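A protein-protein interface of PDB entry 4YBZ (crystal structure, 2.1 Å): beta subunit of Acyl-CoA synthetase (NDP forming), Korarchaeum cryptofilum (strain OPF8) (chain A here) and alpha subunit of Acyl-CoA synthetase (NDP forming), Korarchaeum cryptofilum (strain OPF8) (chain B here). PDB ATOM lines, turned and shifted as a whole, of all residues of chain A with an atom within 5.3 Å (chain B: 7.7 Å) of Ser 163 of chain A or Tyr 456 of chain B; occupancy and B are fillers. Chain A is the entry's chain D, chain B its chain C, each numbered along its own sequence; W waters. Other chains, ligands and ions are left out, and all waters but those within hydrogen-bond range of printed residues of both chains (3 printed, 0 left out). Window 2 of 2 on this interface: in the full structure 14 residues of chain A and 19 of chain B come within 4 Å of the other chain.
Water W1 bridges the side-chain carboxylate (OE2) of Glu 167 of chain A (2.6 Å) and the side-chain hydroxyl (OG) of Ser 267 of chain B (2.9 Å).
Water W2 lies within hydrogen-bond range of the side-chain carboxylate of Asp 160 of chain A (2.7 Å), the side-chain amide nitrogen of Gln 271 of chain B (3.1 Å) and the side-chain hydroxyl of Ser 460 of chain B (3.2 Å).
Water W3 lies within hydrogen-bond range of the backbone carbonyl oxygen (O) of Lys 459 of chain B (2.8 Å), the backbone NH (N) of Gln 159 of chain A (3.2 Å) and the backbone NH (N) of Glu 158 of chain A (3.5 Å).
Arg 152 of chain A touches Gln 271 of chain B.
Gln 159 of chain A touches Tyr 456 of chain B (NE2 to CD2, 3.5 Å).
Gln 159 of chain A touches Lys 459 of chain B.
Ser 460 of chain B touches Gln 159 of chain A.
CG of Gln 271 of chain B touches OD1 of Asp 160 of chain A (3.5 Å).
OD2 of Asp 160 of chain A touches OG of Ser 460 of chain B (3.8 Å).
The side-chain amino group (NZ) of Lys 270 of chain B is in salt-bridge range of the side-chain carboxylate (OE1) of Glu 167 of chain A (2.6 Å).
NE of Arg 152 of chain A is in hydrogen-bond range of OH of Tyr 456 of chain B (3.1 Å).
The side-chain hydroxyl of Tyr 456 of chain B sits at hydrogen-bond distance from the side-chain carboxylate of Asp 160 of chain A, 2.8 Å away.
The side-chain hydroxyl (OH) of Tyr 456 of chain B is in hydrogen-bond range of the side-chain hydroxyl (OG) of Ser 163 of chain A (3.0 Å).
The guanidinium group (NH2) of Arg 152 of chain A sits close to the side-chain amino group (NZ) of Lys 270 of chain B (3.0 Å).
Of the printed residues of chain B, Gln 159 of chain A touches Tyr 456, Lys 459 and Ser 460.
Ser 163 of chain A touches just one residue of chain B: Tyr 456 (3.0 Å).
Lys 166 of chain A touches none of the printed residues of chain B.
Printed residues of chain B within 4 Å of Glu 167 of chain A: Lys 270 (2.6 Å).
Tyr 456 of chain B touches four residues of chain A.
Printed residues of chain A within 4 Å of Lys 459 of chain B: Gln 159 (3.3 Å).
The nearest residue of chain B that does not touch Ser 163 of chain A is Lys 270 of chain B (4.6 Å).
The nearest printed residue of chain A that does not touch Tyr 456 of chain B is Met 164 of chain A (5.6 Å).
The nearest printed residue of chain A that does not touch Ser 460 of chain B is Glu 158 of chain A (5.9 Å).
Of the 11 printed residues of chain A, 5 touch a printed residue of chain B.
Printed residues of chain A that touch a printed residue of chain B: Arg 152, Gln 159, Asp 160, Ser 163 and Glu 167.
Of the 22 printed residues of chain B, 5 touch a printed residue of chain A.
Printed residues of chain B that touch a printed residue of chain A: Lys 270, Gln 271, Tyr 456, Lys 459 and Ser 460.
Among the printed residues, 11 pairs touch across the chains.
Among the printed residues, Asp or Glu carboxylates within 4 Å of a Lys or Arg side-chain nitrogen of the other chain: Glu 167 of chain A with Lys 270 of chain B (2.6 Å).
The guanidinium group of Arg 152 of chain A is in hydrogen-bond range of the side-chain hydroxyl of Ser 163 of chain A (2.9 Å).
The side-chain carboxylate (OE1) of Glu 167 of chain A lies within salt-bridge range of the guanidinium group (NH1) of Arg 152 of chain A (2.9 Å).
O of Gln 159 of chain A sits at hydrogen-bond distance from OG of Ser 163 of chain A (2.9 Å).
The backbone carbonyl oxygen (O) of Asp 160 of chain A lies within hydrogen-bond range of the side-chain hydroxyl (OG) of Ser 163 of chain A (3.2 Å).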
ATOM      1  N   ARG A 152       4.188   0.104  22.980  1.00  0.00           N
ATOM      2  CA  ARG A 152       2.823   0.601  22.846  1.00  0.00           C
ATOM      3  C   ARG A 152       2.201   0.769  24.227  1.00  0.00           C
ATOM      4  O   ARG A 152       2.382  -0.074  25.105  1.00  0.00           O
ATOM      5  CB  ARG A 152       1.968  -0.339  21.995  1.00  0.00           C
ATOM      6  CG  ARG A 152       2.391  -0.446  20.534  1.00  0.00           C
ATOM      7  CD  ARG A 152       2.013   0.793  19.723  1.00  0.00           C
ATOM      8  NE  ARG A 152       2.310   0.593  18.306  1.00  0.00           N
ATOM      9  CZ  ARG A 152       3.491   0.805  17.737  1.00  0.00           C
ATOM     10  NH1 ARG A 152       4.514   1.260  18.447  1.00  0.00           N
ATOM     11  NH2 ARG A 152       3.653   0.576  16.444  1.00  0.00           N
ATOM     12  N   GLU A 158      -5.442  -4.598  18.343  1.00  0.00           N
ATOM     13  CA  GLU A 158      -4.803  -5.519  17.421  1.00  0.00           C
ATOM     14  C   GLU A 158      -3.864  -4.757  16.485  1.00  0.00           C
ATOM     15  O   GLU A 158      -2.797  -5.253  16.116  1.00  0.00           O
ATOM     16  CB  GLU A 158      -5.862  -6.294  16.641  1.00  0.00           C
ATOM     17  CG  GLU A 158      -5.310  -7.169  15.530  1.00  0.00           C
ATOM     18  CD  GLU A 158      -6.318  -8.184  15.028  1.00  0.00           C
ATOM     19  OE1 GLU A 158      -7.394  -8.323  15.650  1.00  0.00           O
ATOM     20  OE2 GLU A 158      -6.033  -8.845  14.008  1.00  0.00           O
ATOM     21  N   GLN A 159      -4.278  -3.552  16.102  1.00  0.00           N
ATOM     22  CA  GLN A 159      -3.466  -2.672  15.267  1.00  0.00           C
ATOM     23  C   GLN A 159      -2.145  -2.315  15.947  1.00  0.00           C
ATOM     24  O   GLN A 159      -1.093  -2.278  15.312  1.00  0.00           O
ATOM     25  CB  GLN A 159      -4.238  -1.395  14.928  1.00  0.00           C
ATOM     26  CG  GLN A 159      -3.466  -0.408  14.063  1.00  0.00           C
ATOM     27  CD  GLN A 159      -3.022  -1.008  12.740  1.00  0.00           C
ATOM     28  OE1 GLN A 159      -3.657  -1.922  12.213  1.00  0.00           O
ATOM     29  NE2 GLN A 159      -1.924  -0.498  12.199  1.00  0.00           N
ATOM     30  N   ASP A 160      -2.205  -1.982  17.232  1.00  0.00           N
ATOM     31  CA  ASP A 160      -0.990  -1.685  17.988  1.00  0.00           C
ATOM     32  C   ASP A 160      -0.050  -2.883  18.017  1.00  0.00           C
ATOM     33  O   ASP A 160       1.148  -2.748  17.762  1.00  0.00           O
ATOM     34  CB  ASP A 160      -1.324  -1.265  19.419  1.00  0.00           C
ATOM     35  CG  ASP A 160      -2.175  -0.024  19.474  1.00  0.00           C
ATOM     36  OD1 ASP A 160      -1.886   0.926  18.720  1.00  0.00           O
ATOM     37  OD2 ASP A 160      -3.136   0.001  20.270  1.00  0.00           O
ATOM     38  N   ALA A 161      -0.599  -4.049  18.337  1.00  0.00           N
ATOM     39  CA  ALA A 161       0.202  -5.261  18.452  1.00  0.00           C
ATOM     40  C   ALA A 161       0.898  -5.583  17.130  1.00  0.00           C
ATOM     41  O   ALA A 161       2.108  -5.810  17.091  1.00  0.00           O
ATOM     42  CB  ALA A 161      -0.669  -6.431  18.893  1.00  0.00           C
ATOM     43  N   GLU A 162       0.138  -5.567  16.041  1.00  0.00           N
ATOM     44  CA  GLU A 162       0.698  -5.889  14.732  1.00  0.00           C
ATOM     45  C   GLU A 162       1.784  -4.905  14.298  1.00  0.00           C
ATOM     46  O   GLU A 162       2.882  -5.313  13.904  1.00  0.00           O
ATOM     47  CB  GLU A 162      -0.408  -5.925  13.674  1.00  0.00           C
ATOM     48  CG  GLU A 162       0.115  -6.225  12.270  1.00  0.00           C
ATOM     49  CD  GLU A 162      -0.851  -7.018  11.406  1.00  0.00           C
ATOM     50  OE1 GLU A 162      -1.923  -7.428  11.901  1.00  0.00           O
ATOM     51  OE2 GLU A 162      -0.530  -7.232  10.218  1.00  0.00           O
ATOM     52  N   SER A 163       1.477  -3.614  14.371  1.00  0.00           N
ATOM     53  CA  SER A 163       2.390  -2.588  13.881  1.00  0.00           C
ATOM     54  C   SER A 163       3.680  -2.535  14.696  1.00  0.00           C
ATOM     55  O   SER A 163       4.758  -2.321  14.141  1.00  0.00           O
ATOM     56  CB  SER A 163       1.706  -1.218  13.893  1.00  0.00           C
ATOM     57  OG  SER A 163       1.407  -0.801  15.215  1.00  0.00           O
ATOM     58  N   MET A 164       3.584  -2.760  16.004  1.00  0.00           N
ATOM     59  CA  MET A 164       4.773  -2.691  16.848  1.00  0.00           C
ATOM     60  C   MET A 164       5.684  -3.886  16.571  1.00  0.00           C
ATOM     61  O   MET A 164       6.902  -3.787  16.724  1.00  0.00           O
ATOM     62  CB  MET A 164       4.398  -2.617  18.331  1.00  0.00           C
ATOM     63  CG  MET A 164       4.166  -3.950  19.020  1.00  0.00           C
ATOM     64  SD  MET A 164       3.507  -3.730  20.686  1.00  0.00           S
ATOM     65  CE  MET A 164       4.959  -3.125  21.552  1.00  0.00           C
ATOM     66  N   ILE A 165       5.100  -5.014  16.167  1.00  0.00           N
ATOM     67  CA  ILE A 165       5.903  -6.157  15.738  1.00  0.00           C
ATOM     68  C   ILE A 165       6.655  -5.825  14.451  1.00  0.00           C
ATOM     69  O   ILE A 165       7.856  -6.061  14.354  1.00  0.00           O
ATOM     70  CB  ILE A 165       5.045  -7.418  15.511  1.00  0.00           C
ATOM     71  CG1 ILE A 165       4.477  -7.917  16.840  1.00  0.00           C
ATOM     72  CG2 ILE A 165       5.872  -8.536  14.860  1.00  0.00           C
ATOM     73  CD1 ILE A 165       3.324  -8.880  16.683  1.00  0.00           C
ATOM     74  N   LYS A 166       5.945  -5.295  13.458  1.00  0.00           N
ATOM     75  CA  LYS A 166       6.570  -4.936  12.185  1.00  0.00           C
ATOM     76  C   LYS A 166       7.604  -3.825  12.338  1.00  0.00           C
ATOM     77  O   LYS A 166       8.468  -3.641  11.480  1.00  0.00           O
ATOM     78  CB  LYS A 166       5.519  -4.495  11.166  1.00  0.00           C
ATOM     79  CG  LYS A 166       4.804  -5.630  10.460  1.00  0.00           C
ATOM     80  CD  LYS A 166       4.110  -5.125   9.203  1.00  0.00           C
ATOM     81  CE  LYS A 166       2.635  -5.483   9.186  1.00  0.00           C
ATOM     82  NZ  LYS A 166       2.407  -6.951   9.113  1.00  0.00           N
ATOM     83  N   GLU A 167       7.499  -3.076  13.430  1.00  0.00           N
ATOM     84  CA  GLU A 167       8.311  -1.886  13.633  1.00  0.00           C
ATOM     85  C   GLU A 167       9.782  -2.199  13.895  1.00  0.00           C
ATOM     86  O   GLU A 167      10.662  -1.488  13.410  1.00  0.00           O
ATOM     87  CB  GLU A 167       7.741  -1.078  14.799  1.00  0.00           C
ATOM     88  CG  GLU A 167       8.346   0.298  14.977  1.00  0.00           C
ATOM     89  CD  GLU A 167       7.824   0.993  16.217  1.00  0.00           C
ATOM     90  OE1 GLU A 167       6.587   1.041  16.392  1.00  0.00           O
ATOM     91  OE2 GLU A 167       8.646   1.483  17.020  1.00  0.00           O
ATOM     92  N   LEU B 232      -9.183  11.657  14.080  1.00  0.00           N
ATOM     93  CA  LEU B 232     -10.136  11.114  13.120  1.00  0.00           C
ATOM     94  C   LEU B 232     -10.658  12.193  12.179  1.00  0.00           C
ATOM     95  O   LEU B 232     -11.079  11.887  11.066  1.00  0.00           O
ATOM     96  CB  LEU B 232     -11.305  10.445  13.841  1.00  0.00           C
ATOM     97  CG  LEU B 232     -10.970   9.171  14.617  1.00  0.00           C
ATOM     98  CD1 LEU B 232     -12.176   8.707  15.408  1.00  0.00           C
ATOM     99  CD2 LEU B 232     -10.499   8.073  13.673  1.00  0.00           C
ATOM    100  N   SER B 267       5.823   6.555  20.464  1.00  0.00           N
ATOM    101  CA  SER B 267       4.843   5.493  20.316  1.00  0.00           C
ATOM    102  C   SER B 267       3.444   6.026  20.594  1.00  0.00           C
ATOM    103  O   SER B 267       2.489   5.699  19.888  1.00  0.00           O
ATOM    104  CB  SER B 267       5.179   4.342  21.258  1.00  0.00           C
ATOM    105  OG  SER B 267       6.433   3.783  20.910  1.00  0.00           O
ATOM    106  N   ALA B 268       3.335   6.854  21.628  1.00  0.00           N
ATOM    107  CA  ALA B 268       2.074   7.494  21.971  1.00  0.00           C
ATOM    108  C   ALA B 268       1.603   8.390  20.833  1.00  0.00           C
ATOM    109  O   ALA B 268       0.409   8.477  20.564  1.00  0.00           O
ATOM    110  CB  ALA B 268       2.217   8.295  23.258  1.00  0.00           C
ATOM    111  N   PHE B 269       2.538   9.069  20.177  1.00  0.00           N
ATOM    112  CA  PHE B 269       2.200   9.919  19.039  1.00  0.00           C
ATOM    113  C   PHE B 269       1.621   9.090  17.900  1.00  0.00           C
ATOM    114  O   PHE B 269       0.639   9.481  17.271  1.00  0.00           O
ATOM    115  CB  PHE B 269       3.435  10.689  18.549  1.00  0.00           C
ATOM    116  CG  PHE B 269       3.901  11.774  19.484  1.00  0.00           C
ATOM    117  CD1 PHE B 269       3.034  12.361  20.393  1.00  0.00           C
ATOM    118  CD2 PHE B 269       5.211  12.216  19.442  1.00  0.00           C
ATOM    119  CE1 PHE B 269       3.469  13.361  21.241  1.00  0.00           C
ATOM    120  CE2 PHE B 269       5.650  13.215  20.288  1.00  0.00           C
ATOM    121  CZ  PHE B 269       4.777  13.786  21.188  1.00  0.00           C
ATOM    122  N   LYS B 270       2.237   7.942  17.649  1.00  0.00           N
ATOM    123  CA  LYS B 270       1.770   7.003  16.635  1.00  0.00           C
ATOM    124  C   LYS B 270       0.352   6.512  16.932  1.00  0.00           C
ATOM    125  O   LYS B 270      -0.515   6.517  16.058  1.00  0.00           O
ATOM    126  CB  LYS B 270       2.758   5.840  16.564  1.00  0.00           C
ATOM    127  CG  LYS B 270       2.571   4.814  15.468  1.00  0.00           C
ATOM    128  CD  LYS B 270       3.938   4.224  15.166  1.00  0.00           C
ATOM    129  CE  LYS B 270       3.893   2.960  14.346  1.00  0.00           C
ATOM    130  NZ  LYS B 270       5.206   2.264  14.501  1.00  0.00           N
ATOM    131  N   GLN B 271       0.111   6.104  18.173  1.00  0.00           N
ATOM    132  CA  GLN B 271      -1.209   5.614  18.570  1.00  0.00           C
ATOM    133  C   GLN B 271      -2.277   6.704  18.525  1.00  0.00           C
ATOM    134  O   GLN B 271      -3.465   6.402  18.415  1.00  0.00           O
ATOM    135  CB  GLN B 271      -1.159   5.010  19.970  1.00  0.00           C
ATOM    136  CG  GLN B 271      -0.303   3.765  20.069  1.00  0.00           C
ATOM    137  CD  GLN B 271      -0.141   3.291  21.493  1.00  0.00           C
ATOM    138  OE1 GLN B 271       0.927   3.439  22.086  1.00  0.00           O
ATOM    139  NE2 GLN B 271      -1.200   2.716  22.050  1.00  0.00           N
ATOM    140  N   SER B 272      -1.852   7.956  18.672  1.00  0.00           N
ATOM    141  CA  SER B 272      -2.757   9.103  18.638  1.00  0.00           C
ATOM    142  C   SER B 272      -3.022   9.619  17.228  1.00  0.00           C
ATOM    143  O   SER B 272      -3.879  10.481  17.032  1.00  0.00           O
ATOM    144  CB  SER B 272      -2.193  10.240  19.486  1.00  0.00           C
ATOM    145  OG  SER B 272      -2.038   9.835  20.832  1.00  0.00           O
ATOM    146  N   GLY B 273      -2.271   9.109  16.256  1.00  0.00           N
ATOM    147  CA  GLY B 273      -2.384   9.560  14.881  1.00  0.00           C
ATOM    148  C   GLY B 273      -1.722  10.909  14.653  1.00  0.00           C
ATOM    149  O   GLY B 273      -2.016  11.599  13.676  1.00  0.00           O
ATOM    150  N   ALA B 449       0.881  11.171   5.035  1.00  0.00           N
ATOM    151  CA  ALA B 449       1.214  10.675   6.364  1.00  0.00           C
ATOM    152  C   ALA B 449       0.012  10.817   7.287  1.00  0.00           C
ATOM    153  O   ALA B 449      -0.259   9.942   8.107  1.00  0.00           O
ATOM    154  CB  ALA B 449       2.412  11.419   6.933  1.00  0.00           C
ATOM    155  N   TYR B 450      -0.706  11.926   7.154  1.00  0.00           N
ATOM    156  CA  TYR B 450      -1.913  12.132   7.941  1.00  0.00           C
ATOM    157  C   TYR B 450      -2.986  11.112   7.569  1.00  0.00           C
ATOM    158  O   TYR B 450      -3.706  10.628   8.438  1.00  0.00           O
ATOM    159  CB  TYR B 450      -2.459  13.549   7.766  1.00  0.00           C
ATOM    160  CG  TYR B 450      -3.757  13.749   8.507  1.00  0.00           C
ATOM    161  CD1 TYR B 450      -3.854  13.427   9.852  1.00  0.00           C
ATOM    162  CD2 TYR B 450      -4.879  14.259   7.874  1.00  0.00           C
ATOM    163  CE1 TYR B 450      -5.030  13.590  10.542  1.00  0.00           C
ATOM    164  CE2 TYR B 450      -6.066  14.435   8.564  1.00  0.00           C
ATOM    165  CZ  TYR B 450      -6.129  14.103   9.899  1.00  0.00           C
ATOM    166  OH  TYR B 450      -7.299  14.272  10.596  1.00  0.00           O
ATOM    167  N   ALA B 451      -3.112  10.812   6.279  1.00  0.00           N
ATOM    168  CA  ALA B 451      -4.061   9.794   5.831  1.00  0.00           C
ATOM    169  C   ALA B 451      -3.761   8.454   6.502  1.00  0.00           C
ATOM    170  O   ALA B 451      -4.661   7.777   7.000  1.00  0.00           O
ATOM    171  CB  ALA B 451      -4.023   9.657   4.318  1.00  0.00           C
ATOM    172  N   ARG B 452      -2.482   8.094   6.549  1.00  0.00           N
ATOM    173  CA  ARG B 452      -2.056   6.857   7.200  1.00  0.00           C
ATOM    174  C   ARG B 452      -2.248   6.901   8.713  1.00  0.00           C
ATOM    175  O   ARG B 452      -2.630   5.906   9.321  1.00  0.00           O
ATOM    176  CB  ARG B 452      -0.595   6.580   6.854  1.00  0.00           C
ATOM    177  CG  ARG B 452      -0.368   6.524   5.356  1.00  0.00           C
ATOM    178  CD  ARG B 452       1.013   6.059   4.973  1.00  0.00           C
ATOM    179  NE  ARG B 452       1.085   5.849   3.527  1.00  0.00           N
ATOM    180  CZ  ARG B 452       2.083   6.241   2.742  1.00  0.00           C
ATOM    181  NH1 ARG B 452       3.126   6.900   3.231  1.00  0.00           N
ATOM    182  NH2 ARG B 452       2.025   5.986   1.441  1.00  0.00           N
ATOM    183  N   ALA B 453      -1.993   8.053   9.322  1.00  0.00           N
ATOM    184  CA  ALA B 453      -2.187   8.209  10.758  1.00  0.00           C
ATOM    185  C   ALA B 453      -3.665   8.036  11.104  1.00  0.00           C
ATOM    186  O   ALA B 453      -4.015   7.355  12.069  1.00  0.00           O
ATOM    187  CB  ALA B 453      -1.683   9.559  11.224  1.00  0.00           C
ATOM    188  N   ARG B 454      -4.521   8.654  10.294  1.00  0.00           N
ATOM    189  CA  ARG B 454      -5.965   8.593  10.480  1.00  0.00           C
ATOM    190  C   ARG B 454      -6.426   7.142  10.370  1.00  0.00           C
ATOM    191  O   ARG B 454      -7.250   6.672  11.157  1.00  0.00           O
ATOM    192  CB  ARG B 454      -6.682   9.441   9.419  1.00  0.00           C
ATOM    193  CG  ARG B 454      -8.204   9.470   9.548  1.00  0.00           C
ATOM    194  CD  ARG B 454      -8.861  10.492   8.612  1.00  0.00           C
ATOM    195  NE  ARG B 454      -8.893  11.877   9.079  1.00  0.00           N
ATOM    196  CZ  ARG B 454      -9.483  12.862   8.401  1.00  0.00           C
ATOM    197  NH1 ARG B 454     -10.081  12.605   7.244  1.00  0.00           N
ATOM    198  NH2 ARG B 454      -9.485  14.105   8.868  1.00  0.00           N
ATOM    199  N   SER B 455      -5.871   6.437   9.389  1.00  0.00           N
ATOM    200  CA  SER B 455      -6.181   5.029   9.179  1.00  0.00           C
ATOM    201  C   SER B 455      -5.686   4.153  10.329  1.00  0.00           C
ATOM    202  O   SER B 455      -6.363   3.203  10.728  1.00  0.00           O
ATOM    203  CB  SER B 455      -5.573   4.555   7.858  1.00  0.00           C
ATOM    204  OG  SER B 455      -5.531   3.142   7.789  1.00  0.00           O
ATOM    205  N   TYR B 456      -4.518   4.484  10.875  1.00  0.00           N
ATOM    206  CA  TYR B 456      -3.990   3.767  12.030  1.00  0.00           C
ATOM    207  C   TYR B 456      -4.979   3.840  13.183  1.00  0.00           C
ATOM    208  O   TYR B 456      -5.322   2.825  13.795  1.00  0.00           O
ATOM    209  CB  TYR B 456      -2.639   4.342  12.468  1.00  0.00           C
ATOM    210  CG  TYR B 456      -1.985   3.548  13.580  1.00  0.00           C
ATOM    211  CD1 TYR B 456      -2.398   3.690  14.900  1.00  0.00           C
ATOM    212  CD2 TYR B 456      -0.965   2.650  13.308  1.00  0.00           C
ATOM    213  CE1 TYR B 456      -1.808   2.961  15.915  1.00  0.00           C
ATOM    214  CE2 TYR B 456      -0.371   1.920  14.313  1.00  0.00           C
ATOM    215  CZ  TYR B 456      -0.794   2.078  15.611  1.00  0.00           C
ATOM    216  OH  TYR B 456      -0.185   1.335  16.592  1.00  0.00           O
ATOM    217  N   VAL B 457      -5.435   5.053  13.471  1.00  0.00           N
ATOM    218  CA  VAL B 457      -6.359   5.284  14.570  1.00  0.00           C
ATOM    219  C   VAL B 457      -7.699   4.587  14.326  1.00  0.00           C
ATOM    220  O   VAL B 457      -8.247   3.964  15.236  1.00  0.00           O
ATOM    221  CB  VAL B 457      -6.575   6.797  14.796  1.00  0.00           C
ATOM    222  CG1 VAL B 457      -7.749   7.056  15.732  1.00  0.00           C
ATOM    223  CG2 VAL B 457      -5.300   7.425  15.356  1.00  0.00           C
ATOM    224  N   MET B 458      -8.229   4.709  13.110  1.00  0.00           N
ATOM    225  CA  MET B 458      -9.483   4.049  12.753  1.00  0.00           C
ATOM    226  C   MET B 458      -9.420   2.560  13.076  1.00  0.00           C
ATOM    227  O   MET B 458     -10.288   2.016  13.767  1.00  0.00           O
ATOM    228  CB  MET B 458      -9.785   4.235  11.265  1.00  0.00           C
ATOM    229  CG  MET B 458     -10.408   5.572  10.897  1.00  0.00           C
ATOM    230  SD  MET B 458     -10.630   5.729   9.111  1.00  0.00           S
ATOM    231  CE  MET B 458     -11.717   7.149   9.017  1.00  0.00           C
ATOM    232  N   LYS B 459      -8.373   1.914  12.576  1.00  0.00           N
ATOM    233  CA  LYS B 459      -8.154   0.495  12.814  1.00  0.00           C
ATOM    234  C   LYS B 459      -8.086   0.209  14.306  1.00  0.00           C
ATOM    235  O   LYS B 459      -8.751  -0.693  14.816  1.00  0.00           O
ATOM    236  CB  LYS B 459      -6.863   0.040  12.141  1.00  0.00           C
ATOM    237  CG  LYS B 459      -6.967  -0.116  10.640  1.00  0.00           C
ATOM    238  CD  LYS B 459      -5.631  -0.515  10.048  1.00  0.00           C
ATOM    239  CE  LYS B 459      -5.623  -0.368   8.541  1.00  0.00           C
ATOM    240  NZ  LYS B 459      -4.609  -1.258   7.916  1.00  0.00           N
ATOM    241  N   SER B 460      -7.282   1.011  14.995  1.00  0.00           N
ATOM    242  CA  SER B 460      -7.039   0.851  16.420  1.00  0.00           C
ATOM    243  C   SER B 460      -8.290   1.025  17.282  1.00  0.00           C
ATOM    244  O   SER B 460      -8.309   0.592  18.432  1.00  0.00           O
ATOM    245  CB  SER B 460      -5.974   1.856  16.859  1.00  0.00           C
ATOM    246  OG  SER B 460      -5.742   1.797  18.252  1.00  0.00           O
ATOM    247  N   LEU B 461      -9.316   1.676  16.741  1.00  0.00           N
ATOM    248  CA  LEU B 461     -10.561   1.889  17.483  1.00  0.00           C
ATOM    249  C   LEU B 461     -11.638   0.869  17.119  1.00  0.00           C
ATOM    250  O   LEU B 461     -12.719   0.873  17.706  1.00  0.00           O
ATOM    251  CB  LEU B 461     -11.096   3.300  17.230  1.00  0.00           C
ATOM    252  CG  LEU B 461     -10.273   4.469  17.780  1.00  0.00           C
ATOM    253  CD1 LEU B 461     -10.932   5.786  17.403  1.00  0.00           C
ATOM    254  CD2 LEU B 461     -10.090   4.372  19.290  1.00  0.00           C
ATOM    255  N   ALA B 462     -11.324  -0.022  16.182  1.00  0.00           N
ATOM    256  CA  ALA B 462     -12.296  -0.992  15.679  1.00  0.00           C
ATOM    257  C   ALA B 462     -12.932  -1.891  16.748  1.00  0.00           C
ATOM    258  O   ALA B 462     -12.268  -2.428  17.639  1.00  0.00           O
ATOM    259  CB  ALA B 462     -11.637  -1.861  14.617  1.00  0.00           C
HETATM  260  O   HOH W   1       8.204   1.940  19.512  1.00  0.00           O
HETATM  261  O   HOH W   2      -4.116   2.361  20.988  1.00  0.00           O
HETATM  262  O   HOH W   3      -7.381  -2.864  16.023  1.00  0.00           O
